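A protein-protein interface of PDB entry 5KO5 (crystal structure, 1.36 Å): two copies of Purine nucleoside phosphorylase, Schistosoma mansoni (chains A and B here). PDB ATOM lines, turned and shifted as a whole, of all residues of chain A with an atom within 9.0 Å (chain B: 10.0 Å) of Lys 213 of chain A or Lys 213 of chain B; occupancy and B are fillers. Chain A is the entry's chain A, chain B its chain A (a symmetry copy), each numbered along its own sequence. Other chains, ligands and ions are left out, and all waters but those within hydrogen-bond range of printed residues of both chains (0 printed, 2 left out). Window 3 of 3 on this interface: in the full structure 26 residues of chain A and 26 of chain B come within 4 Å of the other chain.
Hydrophobic or aromatic side chains of chain B that line the printed part of chain A: Met 210 and Leu 214. Of the 19 printed residues of chain A, 5 touch a printed residue of chain B. Among the printed residues, no Asp or Glu carboxylate lies within 4 Å of a Lys or Arg side-chain nitrogen of the other chain.
The backbone NH (N) of Val 193 of chain A is in hydrogen-bond range of the side-chain carboxylate (OD2) of Asp 217 of chain A (2.8 Å).
Ile 138 of chain A touches Glu 207 of chain B, but with the chains exchanged Glu 207 of chain A does not touch Ile 138 of chain B (15.4 Å). Ile 138 of chain A touches Met 210 of chain B, but with the chains exchanged Met 210 of chain A does not touch Ile 138 of chain B (10.5 Å). Leu 214 of chain A touches Met 210 of chain B, but with the chains exchanged Met 210 of chain A does not touch Leu 214 of chain B (6.9 Å). Leu 214 of chain A touches its own counterpart, Leu 214 of chain B. Of the 8 pairs that touch across the chains among the printed residues, 2 have their exchanged pair printed and touching as well.
Ile 138 of chain A touches Glu 207 of chain B (C to OE2, 3.8 Å). Ile 138 of chain A touches Met 210 of chain B (CG2 to SD, 3.8 Å). Asp 206 of chain B touches Val 193 of chain A (OD1 to CG2, 3.4 Å). O of Lys 213 of chain A touches CD of Lys 213 of chain B (3.96 Å). Met 210 of chain B touches Leu 214 of chain A (SD to CD1, 3.6 Å). NZ of Lys 213 of chain B touches O of Leu 214 of chain A (3.9 Å). Leu 214 of chain B touches Leu 214 of chain A (CD2 to CD2, 3.7 Å). Lys 213 of chain B touches Gly 215 of chain A (NZ to CA, 3.8 Å).
Of the printed residues of chain B, Ile 138 of chain A touches Glu 207 and Met 210. Of the printed residues of chain B, Val 193 of chain A touches Asp 206 (3.4 Å). Asp 206 of chain A touches none of the printed residues of chain B. No residue of chain B comes within 4 Å of Leu 212 of chain A. Of chain B, only Lys 213 (3.96 Å) comes within 4 Å of Lys 213 of chain A. Leu 214 of chain A touches just these residues of chain B: Met 210, Lys 213 and Leu 214. Gly 215 of chain A touches just one residue of chain B: Lys 213. Of the printed residues of chain A, Asp 206 of chain B touches Val 193. Printed residues of chain A within 4 Å of Glu 207 of chain B: Ile 138 (3.8 Å). Leu 211 of chain B touches none of the printed residues of chain A. Of chain A, only Lys 213, Leu 214 and Gly 215 come within 4 Å of Lys 213 of chain B.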
ATOM      1  N   ILE A 122     -18.820   7.086 -13.476  1.00  0.00           N
ATOM      2  CA  ILE A 122     -17.966   5.912 -13.349  1.00  0.00           C
ATOM      3  C   ILE A 122     -18.688   4.787 -12.618  1.00  0.00           C
ATOM      4  O   ILE A 122     -18.696   3.644 -13.073  1.00  0.00           O
ATOM      5  CB  ILE A 122     -16.644   6.272 -12.635  1.00  0.00           C
ATOM      6  CG1 ILE A 122     -15.884   7.367 -13.385  1.00  0.00           C
ATOM      7  CG2 ILE A 122     -15.780   5.027 -12.469  1.00  0.00           C
ATOM      8  CD1 ILE A 122     -15.349   6.932 -14.755  1.00  0.00           C
ATOM      9  N   ASN A 123     -19.290   5.103 -11.469  1.00  0.00           N
ATOM     10  CA  ASN A 123     -20.085   4.141 -10.716  1.00  0.00           C
ATOM     11  C   ASN A 123     -21.181   3.559 -11.598  1.00  0.00           C
ATOM     12  O   ASN A 123     -21.849   4.277 -12.345  1.00  0.00           O
ATOM     13  CB  ASN A 123     -20.734   4.854  -9.521  1.00  0.00           C
ATOM     14  CG  ASN A 123     -21.359   3.883  -8.521  1.00  0.00           C
ATOM     15  OD1 ASN A 123     -22.277   3.136  -8.846  1.00  0.00           O
ATOM     16  ND2 ASN A 123     -20.855   3.904  -7.293  1.00  0.00           N
ATOM     17  N   ARG A 124     -21.383   2.246 -11.485  1.00  0.00           N
ATOM     18  CA  ARG A 124     -22.346   1.577 -12.346  1.00  0.00           C
ATOM     19  C   ARG A 124     -23.774   2.017 -12.104  1.00  0.00           C
ATOM     20  O   ARG A 124     -24.616   1.840 -12.989  1.00  0.00           O
ATOM     21  CB  ARG A 124     -22.258   0.059 -12.163  1.00  0.00           C
ATOM     22  CG  ARG A 124     -22.241  -0.719 -13.484  1.00  0.00           C
ATOM     23  CD  ARG A 124     -20.945  -0.567 -14.260  1.00  0.00           C
ATOM     24  NE  ARG A 124     -20.049   0.463 -13.759  1.00  0.00           N
ATOM     25  CZ  ARG A 124     -19.132   0.285 -12.818  1.00  0.00           C
ATOM     26  NH1 ARG A 124     -18.932  -0.917 -12.279  1.00  0.00           N
ATOM     27  NH2 ARG A 124     -18.422   1.329 -12.434  1.00  0.00           N
ATOM     28  N   ILE A 138     -11.088  13.249  -5.496  1.00  0.00           N
ATOM     29  CA  ILE A 138      -9.710  12.835  -5.749  1.00  0.00           C
ATOM     30  C   ILE A 138      -9.122  13.847  -6.718  1.00  0.00           C
ATOM     31  O   ILE A 138      -9.551  13.943  -7.875  1.00  0.00           O
ATOM     32  CB  ILE A 138      -9.607  11.409  -6.291  1.00  0.00           C
ATOM     33  CG1 ILE A 138     -10.179  10.441  -5.247  1.00  0.00           C
ATOM     34  CG2 ILE A 138      -8.140  11.078  -6.598  1.00  0.00           C
ATOM     35  CD1 ILE A 138     -10.155   8.995  -5.647  1.00  0.00           C
ATOM     36  N   VAL A 193     -18.035  10.447  -5.031  1.00  0.00           N
ATOM     37  CA  VAL A 193     -16.701  11.041  -5.020  1.00  0.00           C
ATOM     38  C   VAL A 193     -16.355  11.498  -6.431  1.00  0.00           C
ATOM     39  O   VAL A 193     -16.507  10.735  -7.395  1.00  0.00           O
ATOM     40  CB  VAL A 193     -15.665  10.016  -4.528  1.00  0.00           C
ATOM     41  CG1 VAL A 193     -14.236  10.559  -4.685  1.00  0.00           C
ATOM     42  CG2 VAL A 193     -15.947   9.629  -3.085  1.00  0.00           C
ATOM     43  N   PRO A 205     -10.949   5.517 -22.076  1.00  0.00           N
ATOM     44  CA  PRO A 205     -11.579   4.303 -21.531  1.00  0.00           C
ATOM     45  C   PRO A 205     -10.756   3.652 -20.434  1.00  0.00           C
ATOM     46  O   PRO A 205     -11.307   3.165 -19.440  1.00  0.00           O
ATOM     47  CB  PRO A 205     -11.736   3.398 -22.763  1.00  0.00           C
ATOM     48  CG  PRO A 205     -11.893   4.358 -23.906  1.00  0.00           C
ATOM     49  CD  PRO A 205     -11.030   5.571 -23.550  1.00  0.00           C
ATOM     50  N   ASP A 206      -9.433   3.639 -20.582  1.00  0.00           N
ATOM     51  CA  ASP A 206      -8.611   3.007 -19.561  1.00  0.00           C
ATOM     52  C   ASP A 206      -8.425   3.881 -18.334  1.00  0.00           C
ATOM     53  O   ASP A 206      -8.278   3.347 -17.228  1.00  0.00           O
ATOM     54  CB  ASP A 206      -7.294   2.554 -20.175  1.00  0.00           C
ATOM     55  CG  ASP A 206      -7.524   1.512 -21.222  1.00  0.00           C
ATOM     56  OD1 ASP A 206      -7.935   0.400 -20.836  1.00  0.00           O
ATOM     57  OD2 ASP A 206      -7.346   1.808 -22.422  1.00  0.00           O
ATOM     58  N   GLU A 207      -8.437   5.207 -18.498  1.00  0.00           N
ATOM     59  CA  GLU A 207      -8.510   6.081 -17.331  1.00  0.00           C
ATOM     60  C   GLU A 207      -9.810   5.869 -16.570  1.00  0.00           C
ATOM     61  O   GLU A 207      -9.805   5.788 -15.334  1.00  0.00           O
ATOM     62  CB  GLU A 207      -8.353   7.541 -17.757  1.00  0.00           C
ATOM     63  CG  GLU A 207      -6.926   7.831 -18.231  1.00  0.00           C
ATOM     64  CD  GLU A 207      -6.809   9.046 -19.115  1.00  0.00           C
ATOM     65  OE1 GLU A 207      -7.813   9.745 -19.355  1.00  0.00           O
ATOM     66  OE2 GLU A 207      -5.688   9.292 -19.599  1.00  0.00           O
ATOM     67  N   SER A 208     -10.931   5.743 -17.287  1.00  0.00           N
ATOM     68  CA  SER A 208     -12.194   5.465 -16.609  1.00  0.00           C
ATOM     69  C   SER A 208     -12.120   4.164 -15.827  1.00  0.00           C
ATOM     70  O   SER A 208     -12.582   4.092 -14.683  1.00  0.00           O
ATOM     71  CB  SER A 208     -13.327   5.407 -17.625  1.00  0.00           C
ATOM     72  OG  SER A 208     -13.502   6.684 -18.208  1.00  0.00           O
ATOM     73  N   ASN A 209     -11.550   3.120 -16.429  1.00  0.00           N
ATOM     74  CA  ASN A 209     -11.444   1.840 -15.733  1.00  0.00           C
ATOM     75  C   ASN A 209     -10.567   1.951 -14.496  1.00  0.00           C
ATOM     76  O   ASN A 209     -10.858   1.341 -13.463  1.00  0.00           O
ATOM     77  CB  ASN A 209     -10.937   0.756 -16.680  1.00  0.00           C
ATOM     78  CG  ASN A 209     -12.051  -0.155 -17.137  1.00  0.00           C
ATOM     79  OD1 ASN A 209     -12.620   0.023 -18.213  1.00  0.00           O
ATOM     80  ND2 ASN A 209     -12.403  -1.118 -16.290  1.00  0.00           N
ATOM     81  N   MET A 210      -9.498   2.743 -14.573  1.00  0.00           N
ATOM     82  CA  MET A 210      -8.678   2.980 -13.395  1.00  0.00           C
ATOM     83  C   MET A 210      -9.479   3.684 -12.307  1.00  0.00           C
ATOM     84  O   MET A 210      -9.419   3.301 -11.131  1.00  0.00           O
ATOM     85  CB  MET A 210      -7.459   3.814 -13.776  1.00  0.00           C
ATOM     86  CG  MET A 210      -6.603   4.156 -12.581  1.00  0.00           C
ATOM     87  SD  MET A 210      -5.226   5.226 -13.004  1.00  0.00           S
ATOM     88  CE  MET A 210      -6.072   6.743 -13.357  1.00  0.00           C
ATOM     89  N   LEU A 211     -10.253   4.706 -12.688  1.00  0.00           N
ATOM     90  CA  LEU A 211     -11.035   5.453 -11.701  1.00  0.00           C
ATOM     91  C   LEU A 211     -12.049   4.561 -11.009  1.00  0.00           C
ATOM     92  O   LEU A 211     -12.322   4.719  -9.810  1.00  0.00           O
ATOM     93  CB  LEU A 211     -11.746   6.616 -12.381  1.00  0.00           C
ATOM     94  CG  LEU A 211     -10.795   7.658 -12.956  1.00  0.00           C
ATOM     95  CD1 LEU A 211     -11.574   8.790 -13.608  1.00  0.00           C
ATOM     96  CD2 LEU A 211      -9.838   8.192 -11.879  1.00  0.00           C
ATOM     97  N   LEU A 212     -12.630   3.625 -11.750  1.00  0.00           N
ATOM     98  CA  LEU A 212     -13.508   2.639 -11.136  1.00  0.00           C
ATOM     99  C   LEU A 212     -12.780   1.878 -10.031  1.00  0.00           C
ATOM    100  O   LEU A 212     -13.285   1.756  -8.909  1.00  0.00           O
ATOM    101  CB  LEU A 212     -14.029   1.690 -12.208  1.00  0.00           C
ATOM    102  CG  LEU A 212     -14.889   0.558 -11.671  1.00  0.00           C
ATOM    103  CD1 LEU A 212     -15.916   1.149 -10.728  1.00  0.00           C
ATOM    104  CD2 LEU A 212     -15.548  -0.166 -12.823  1.00  0.00           C
ATOM    105  N   LYS A 213     -11.577   1.379 -10.327  1.00  0.00           N
ATOM    106  CA  LYS A 213     -10.815   0.633  -9.327  1.00  0.00           C
ATOM    107  C   LYS A 213     -10.448   1.496  -8.126  1.00  0.00           C
ATOM    108  O   LYS A 213     -10.252   0.969  -7.024  1.00  0.00           O
ATOM    109  CB  LYS A 213      -9.545   0.068  -9.965  1.00  0.00           C
ATOM    110  CG  LYS A 213      -9.829  -0.956 -11.041  1.00  0.00           C
ATOM    111  CD  LYS A 213      -8.595  -1.333 -11.834  1.00  0.00           C
ATOM    112  CE  LYS A 213      -8.979  -2.305 -12.935  1.00  0.00           C
ATOM    113  NZ  LYS A 213      -7.959  -2.380 -14.000  1.00  0.00           N
ATOM    114  N   LEU A 214     -10.352   2.806  -8.307  1.00  0.00           N
ATOM    115  CA  LEU A 214      -9.903   3.712  -7.258  1.00  0.00           C
ATOM    116  C   LEU A 214     -11.046   4.306  -6.441  1.00  0.00           C
ATOM    117  O   LEU A 214     -10.808   5.234  -5.659  1.00  0.00           O
ATOM    118  CB  LEU A 214      -9.029   4.819  -7.844  1.00  0.00           C
ATOM    119  CG  LEU A 214      -7.741   4.266  -8.435  1.00  0.00           C
ATOM    120  CD1 LEU A 214      -6.854   5.390  -8.921  1.00  0.00           C
ATOM    121  CD2 LEU A 214      -7.039   3.413  -7.386  1.00  0.00           C
ATOM    122  N   GLY A 215     -12.267   3.788  -6.602  1.00  0.00           N
ATOM    123  CA  GLY A 215     -13.418   4.226  -5.843  1.00  0.00           C
ATOM    124  C   GLY A 215     -14.196   5.386  -6.434  1.00  0.00           C
ATOM    125  O   GLY A 215     -15.328   5.634  -6.002  1.00  0.00           O
ATOM    126  N   CYS A 216     -13.633   6.082  -7.422  1.00  0.00           N
ATOM    127  CA  CYS A 216     -14.259   7.288  -7.955  1.00  0.00           C
ATOM    128  C   CYS A 216     -15.637   6.992  -8.532  1.00  0.00           C
ATOM    129  O   CYS A 216     -15.838   6.002  -9.238  1.00  0.00           O
ATOM    130  CB  CYS A 216     -13.400   7.888  -9.064  1.00  0.00           C
ATOM    131  SG  CYS A 216     -11.729   8.318  -8.589  1.00  0.00           S
ATOM    132  N   ASP A 217     -16.584   7.880  -8.252  1.00  0.00           N
ATOM    133  CA  ASP A 217     -17.936   7.739  -8.774  1.00  0.00           C
ATOM    134  C   ASP A 217     -18.195   8.552 -10.029  1.00  0.00           C
ATOM    135  O   ASP A 217     -18.980   8.110 -10.874  1.00  0.00           O
ATOM    136  CB  ASP A 217     -18.956   8.120  -7.698  1.00  0.00           C
ATOM    137  CG  ASP A 217     -18.837   7.236  -6.469  1.00  0.00           C
ATOM    138  OD1 ASP A 217     -19.082   6.021  -6.615  1.00  0.00           O
ATOM    139  OD2 ASP A 217     -18.479   7.722  -5.380  1.00  0.00           O
ATOM    140  N   ILE A 248     -17.967   4.097 -18.157  1.00  0.00           N
ATOM    141  CA  ILE A 248     -17.626   2.679 -18.092  1.00  0.00           C
ATOM    142  C   ILE A 248     -18.490   1.891 -19.064  1.00  0.00           C
ATOM    143  O   ILE A 248     -17.996   1.061 -19.833  1.00  0.00           O
ATOM    144  CB  ILE A 248     -17.768   2.159 -16.647  1.00  0.00           C
ATOM    145  CG1 ILE A 248     -16.678   2.747 -15.738  1.00  0.00           C
ATOM    146  CG2 ILE A 248     -17.760   0.624 -16.615  1.00  0.00           C
ATOM    147  CD1 ILE A 248     -15.260   2.340 -16.107  1.00  0.00           C
ATOM    148  N   ILE B 122      -1.196   6.068   6.362  1.00  0.00           N
ATOM    149  CA  ILE B 122      -2.227   5.385   5.591  1.00  0.00           C
ATOM    150  C   ILE B 122      -2.373   3.936   6.037  1.00  0.00           C
ATOM    151  O   ILE B 122      -3.481   3.461   6.282  1.00  0.00           O
ATOM    152  CB  ILE B 122      -1.922   5.466   4.078  1.00  0.00           C
ATOM    153  CG1 ILE B 122      -1.821   6.917   3.605  1.00  0.00           C
ATOM    154  CG2 ILE B 122      -2.983   4.710   3.287  1.00  0.00           C
ATOM    155  CD1 ILE B 122      -3.146   7.689   3.664  1.00  0.00           C
ATOM    156  N   ASN B 123      -1.250   3.218   6.133  1.00  0.00           N
ATOM    157  CA  ASN B 123      -1.243   1.847   6.629  1.00  0.00           C
ATOM    158  C   ASN B 123      -1.880   1.784   8.010  1.00  0.00           C
ATOM    159  O   ASN B 123      -1.620   2.625   8.873  1.00  0.00           O
ATOM    160  CB  ASN B 123       0.209   1.359   6.728  1.00  0.00           C
ATOM    161  CG  ASN B 123       0.312  -0.145   6.973  1.00  0.00           C
ATOM    162  OD1 ASN B 123      -0.153  -0.660   7.985  1.00  0.00           O
ATOM    163  ND2 ASN B 123       0.935  -0.849   6.035  1.00  0.00           N
ATOM    164  N   ARG B 124      -2.702   0.757   8.225  1.00  0.00           N
ATOM    165  CA  ARG B 124      -3.430   0.651   9.480  1.00  0.00           C
ATOM    166  C   ARG B 124      -2.530   0.438  10.678  1.00  0.00           C
ATOM    167  O   ARG B 124      -2.952   0.716  11.804  1.00  0.00           O
ATOM    168  CB  ARG B 124      -4.444  -0.494   9.413  1.00  0.00           C
ATOM    169  CG  ARG B 124      -5.831  -0.118   9.948  1.00  0.00           C
ATOM    170  CD  ARG B 124      -6.592   0.834   9.043  1.00  0.00           C
ATOM    171  NE  ARG B 124      -5.805   1.418   7.968  1.00  0.00           N
ATOM    172  CZ  ARG B 124      -5.628   0.875   6.772  1.00  0.00           C
ATOM    173  NH1 ARG B 124      -6.227  -0.270   6.446  1.00  0.00           N
ATOM    174  NH2 ARG B 124      -4.847   1.502   5.912  1.00  0.00           N
ATOM    175  N   ILE B 138       5.881   6.722  -4.171  1.00  0.00           N
ATOM    176  CA  ILE B 138       5.008   6.949  -5.321  1.00  0.00           C
ATOM    177  C   ILE B 138       4.965   8.451  -5.546  1.00  0.00           C
ATOM    178  O   ILE B 138       4.449   9.204  -4.712  1.00  0.00           O
ATOM    179  CB  ILE B 138       3.608   6.367  -5.129  1.00  0.00           C
ATOM    180  CG1 ILE B 138       3.724   4.848  -4.950  1.00  0.00           C
ATOM    181  CG2 ILE B 138       2.735   6.710  -6.344  1.00  0.00           C
ATOM    182  CD1 ILE B 138       2.420   4.136  -4.739  1.00  0.00           C
ATOM    183  N   PHE B 140       3.576  11.219  -7.292  1.00  0.00           N
ATOM    184  CA  PHE B 140       2.500  11.705  -8.148  1.00  0.00           C
ATOM    185  C   PHE B 140       2.923  12.893  -8.997  1.00  0.00           C
ATOM    186  O   PHE B 140       2.600  12.897 -10.200  1.00  0.00           O
ATOM    187  CB  PHE B 140       1.228  11.956  -7.331  1.00  0.00           C
ATOM    188  CG  PHE B 140       0.573  10.686  -6.853  1.00  0.00           C
ATOM    189  CD1 PHE B 140      -0.193   9.919  -7.726  1.00  0.00           C
ATOM    190  CD2 PHE B 140       0.756  10.236  -5.556  1.00  0.00           C
ATOM    191  CE1 PHE B 140      -0.786   8.740  -7.295  1.00  0.00           C
ATOM    192  CE2 PHE B 140       0.169   9.064  -5.124  1.00  0.00           C
ATOM    193  CZ  PHE B 140      -0.609   8.320  -5.993  1.00  0.00           C
ATOM    194  N   PRO B 205     -10.028  12.811   2.502  1.00  0.00           N
ATOM    195  CA  PRO B 205     -10.382  11.449   2.940  1.00  0.00           C
ATOM    196  C   PRO B 205     -10.424  10.454   1.795  1.00  0.00           C
ATOM    197  O   PRO B 205      -9.996   9.303   1.949  1.00  0.00           O
ATOM    198  CB  PRO B 205     -11.754  11.635   3.609  1.00  0.00           C
ATOM    199  CG  PRO B 205     -11.717  13.038   4.139  1.00  0.00           C
ATOM    200  CD  PRO B 205     -10.877  13.837   3.140  1.00  0.00           C
ATOM    201  N   ASP B 206     -10.924  10.870   0.634  1.00  0.00           N
ATOM    202  CA  ASP B 206     -10.998   9.938  -0.482  1.00  0.00           C
ATOM    203  C   ASP B 206      -9.661   9.743  -1.173  1.00  0.00           C
ATOM    204  O   ASP B 206      -9.409   8.654  -1.704  1.00  0.00           O
ATOM    205  CB  ASP B 206     -12.104  10.370  -1.433  1.00  0.00           C
ATOM    206  CG  ASP B 206     -13.439  10.316  -0.761  1.00  0.00           C
ATOM    207  OD1 ASP B 206     -13.882   9.188  -0.470  1.00  0.00           O
ATOM    208  OD2 ASP B 206     -14.020  11.385  -0.481  1.00  0.00           O
ATOM    209  N   GLU B 207      -8.797  10.761  -1.171  1.00  0.00           N
ATOM    210  CA  GLU B 207      -7.419  10.544  -1.601  1.00  0.00           C
ATOM    211  C   GLU B 207      -6.710   9.558  -0.684  1.00  0.00           C
ATOM    212  O   GLU B 207      -6.006   8.657  -1.159  1.00  0.00           O
ATOM    213  CB  GLU B 207      -6.672  11.876  -1.663  1.00  0.00           C
ATOM    214  CG  GLU B 207      -7.184  12.749  -2.811  1.00  0.00           C
ATOM    215  CD  GLU B 207      -6.885  14.216  -2.646  1.00  0.00           C
ATOM    216  OE1 GLU B 207      -6.223  14.615  -1.668  1.00  0.00           O
ATOM    217  OE2 GLU B 207      -7.344  14.991  -3.506  1.00  0.00           O
ATOM    218  N   SER B 208      -6.907   9.689   0.631  1.00  0.00           N
ATOM    219  CA  SER B 208      -6.308   8.725   1.550  1.00  0.00           C
ATOM    220  C   SER B 208      -6.791   7.314   1.254  1.00  0.00           C
ATOM    221  O   SER B 208      -5.996   6.368   1.243  1.00  0.00           O
ATOM    222  CB  SER B 208      -6.637   9.104   2.988  1.00  0.00           C
ATOM    223  OG  SER B 208      -6.019  10.336   3.303  1.00  0.00           O
ATOM    224  N   ASN B 209      -8.093   7.150   1.017  1.00  0.00           N
ATOM    225  CA  ASN B 209      -8.622   5.821   0.722  1.00  0.00           C
ATOM    226  C   ASN B 209      -8.041   5.264  -0.568  1.00  0.00           C
ATOM    227  O   ASN B 209      -7.757   4.067  -0.663  1.00  0.00           O
ATOM    228  CB  ASN B 209     -10.147   5.850   0.679  1.00  0.00           C
ATOM    229  CG  ASN B 209     -10.755   5.265   1.931  1.00  0.00           C
ATOM    230  OD1 ASN B 209     -11.120   5.985   2.859  1.00  0.00           O
ATOM    231  ND2 ASN B 209     -10.824   3.938   1.983  1.00  0.00           N
ATOM    232  N   MET B 210      -7.837   6.122  -1.567  1.00  0.00           N
ATOM    233  CA  MET B 210      -7.183   5.678  -2.789  1.00  0.00           C
ATOM    234  C   MET B 210      -5.757   5.219  -2.507  1.00  0.00           C
ATOM    235  O   MET B 210      -5.326   4.166  -2.994  1.00  0.00           O
ATOM    236  CB  MET B 210      -7.182   6.810  -3.811  1.00  0.00           C
ATOM    237  CG  MET B 210      -6.452   6.436  -5.078  1.00  0.00           C
ATOM    238  SD  MET B 210      -6.352   7.796  -6.243  1.00  0.00           S
ATOM    239  CE  MET B 210      -5.216   8.872  -5.412  1.00  0.00           C
ATOM    240  N   LEU B 211      -5.019   5.992  -1.705  1.00  0.00           N
ATOM    241  CA  LEU B 211      -3.630   5.637  -1.405  1.00  0.00           C
ATOM    242  C   LEU B 211      -3.543   4.303  -0.687  1.00  0.00           C
ATOM    243  O   LEU B 211      -2.604   3.524  -0.905  1.00  0.00           O
ATOM    244  CB  LEU B 211      -2.993   6.728  -0.552  1.00  0.00           C
ATOM    245  CG  LEU B 211      -2.879   8.069  -1.265  1.00  0.00           C
ATOM    246  CD1 LEU B 211      -2.226   9.101  -0.359  1.00  0.00           C
ATOM    247  CD2 LEU B 211      -2.114   7.931  -2.590  1.00  0.00           C
ATOM    248  N   LEU B 212      -4.506   4.026   0.185  1.00  0.00           N
ATOM    249  CA  LEU B 212      -4.576   2.715   0.812  1.00  0.00           C
ATOM    250  C   LEU B 212      -4.664   1.614  -0.241  1.00  0.00           C
ATOM    251  O   LEU B 212      -3.906   0.638  -0.201  1.00  0.00           O
ATOM    252  CB  LEU B 212      -5.771   2.670   1.757  1.00  0.00           C
ATOM    253  CG  LEU B 212      -6.000   1.315   2.406  1.00  0.00           C
ATOM    254  CD1 LEU B 212      -4.678   0.823   2.957  1.00  0.00           C
ATOM    255  CD2 LEU B 212      -7.039   1.447   3.496  1.00  0.00           C
ATOM    256  N   LYS B 213      -5.572   1.769  -1.209  1.00  0.00           N
ATOM    257  CA  LYS B 213      -5.725   0.758  -2.254  1.00  0.00           C
ATOM    258  C   LYS B 213      -4.466   0.617  -3.101  1.00  0.00           C
ATOM    259  O   LYS B 213      -4.225  -0.452  -3.677  1.00  0.00           O
ATOM    260  CB  LYS B 213      -6.912   1.118  -3.148  1.00  0.00           C
ATOM    261  CG  LYS B 213      -8.235   1.083  -2.416  1.00  0.00           C
ATOM    262  CD  LYS B 213      -9.371   1.671  -3.227  1.00  0.00           C
ATOM    263  CE  LYS B 213     -10.642   1.663  -2.397  1.00  0.00           C
ATOM    264  NZ  LYS B 213     -11.662   2.592  -2.922  1.00  0.00           N
ATOM    265  N   LEU B 214      -3.656   1.664  -3.193  1.00  0.00           N
ATOM    266  CA  LEU B 214      -2.486   1.677  -4.060  1.00  0.00           C
ATOM    267  C   LEU B 214      -1.205   1.244  -3.354  1.00  0.00           C
ATOM    268  O   LEU B 214      -0.119   1.403  -3.924  1.00  0.00           O
ATOM    269  CB  LEU B 214      -2.308   3.051  -4.701  1.00  0.00           C
ATOM    270  CG  LEU B 214      -3.464   3.392  -5.630  1.00  0.00           C
ATOM    271  CD1 LEU B 214      -3.217   4.713  -6.322  1.00  0.00           C
ATOM    272  CD2 LEU B 214      -3.646   2.260  -6.633  1.00  0.00           C
ATOM    273  N   GLY B 215      -1.312   0.700  -2.138  1.00  0.00           N
ATOM    274  CA  GLY B 215      -0.177   0.199  -1.393  1.00  0.00           C
ATOM    275  C   GLY B 215       0.533   1.209  -0.513  1.00  0.00           C
ATOM    276  O   GLY B 215       1.322   0.806   0.351  1.00  0.00           O
ATOM    277  N   CYS B 216       0.257   2.502  -0.690  1.00  0.00           N
ATOM    278  CA  CYS B 216       0.991   3.541   0.025  1.00  0.00           C
ATOM    279  C   CYS B 216       0.835   3.396   1.533  1.00  0.00           C
ATOM    280  O   CYS B 216      -0.259   3.151   2.044  1.00  0.00           O
ATOM    281  CB  CYS B 216       0.481   4.923  -0.373  1.00  0.00           C
ATOM    282  SG  CYS B 216       0.583   5.301  -2.119  1.00  0.00           S
ATOM    283  N   ASP B 217       1.938   3.581   2.249  1.00  0.00           N
ATOM    284  CA  ASP B 217       1.921   3.511   3.703  1.00  0.00           C
ATOM    285  C   ASP B 217       1.812   4.866   4.380  1.00  0.00           C
ATOM    286  O   ASP B 217       1.206   4.949   5.452  1.00  0.00           O
ATOM    287  CB  ASP B 217       3.170   2.786   4.209  1.00  0.00           C
ATOM    288  CG  ASP B 217       3.253   1.367   3.675  1.00  0.00           C
ATOM    289  OD1 ASP B 217       2.356   0.573   4.024  1.00  0.00           O
ATOM    290  OD2 ASP B 217       4.172   1.042   2.899  1.00  0.00           O
ATOM    291  N   ILE B 248      -6.517   7.434   7.540  1.00  0.00           N
ATOM    292  CA  ILE B 248      -7.608   6.500   7.279  1.00  0.00           C
ATOM    293  C   ILE B 248      -8.521   6.413   8.493  1.00  0.00           C
ATOM    294  O   ILE B 248      -9.748   6.492   8.379  1.00  0.00           O
ATOM    295  CB  ILE B 248      -7.049   5.118   6.884  1.00  0.00           C
ATOM    296  CG1 ILE B 248      -6.389   5.165   5.497  1.00  0.00           C
ATOM    297  CG2 ILE B 248      -8.146   4.045   6.948  1.00  0.00           C
ATOM    298  CD1 ILE B 248      -7.340   5.486   4.354  1.00  0.00           C
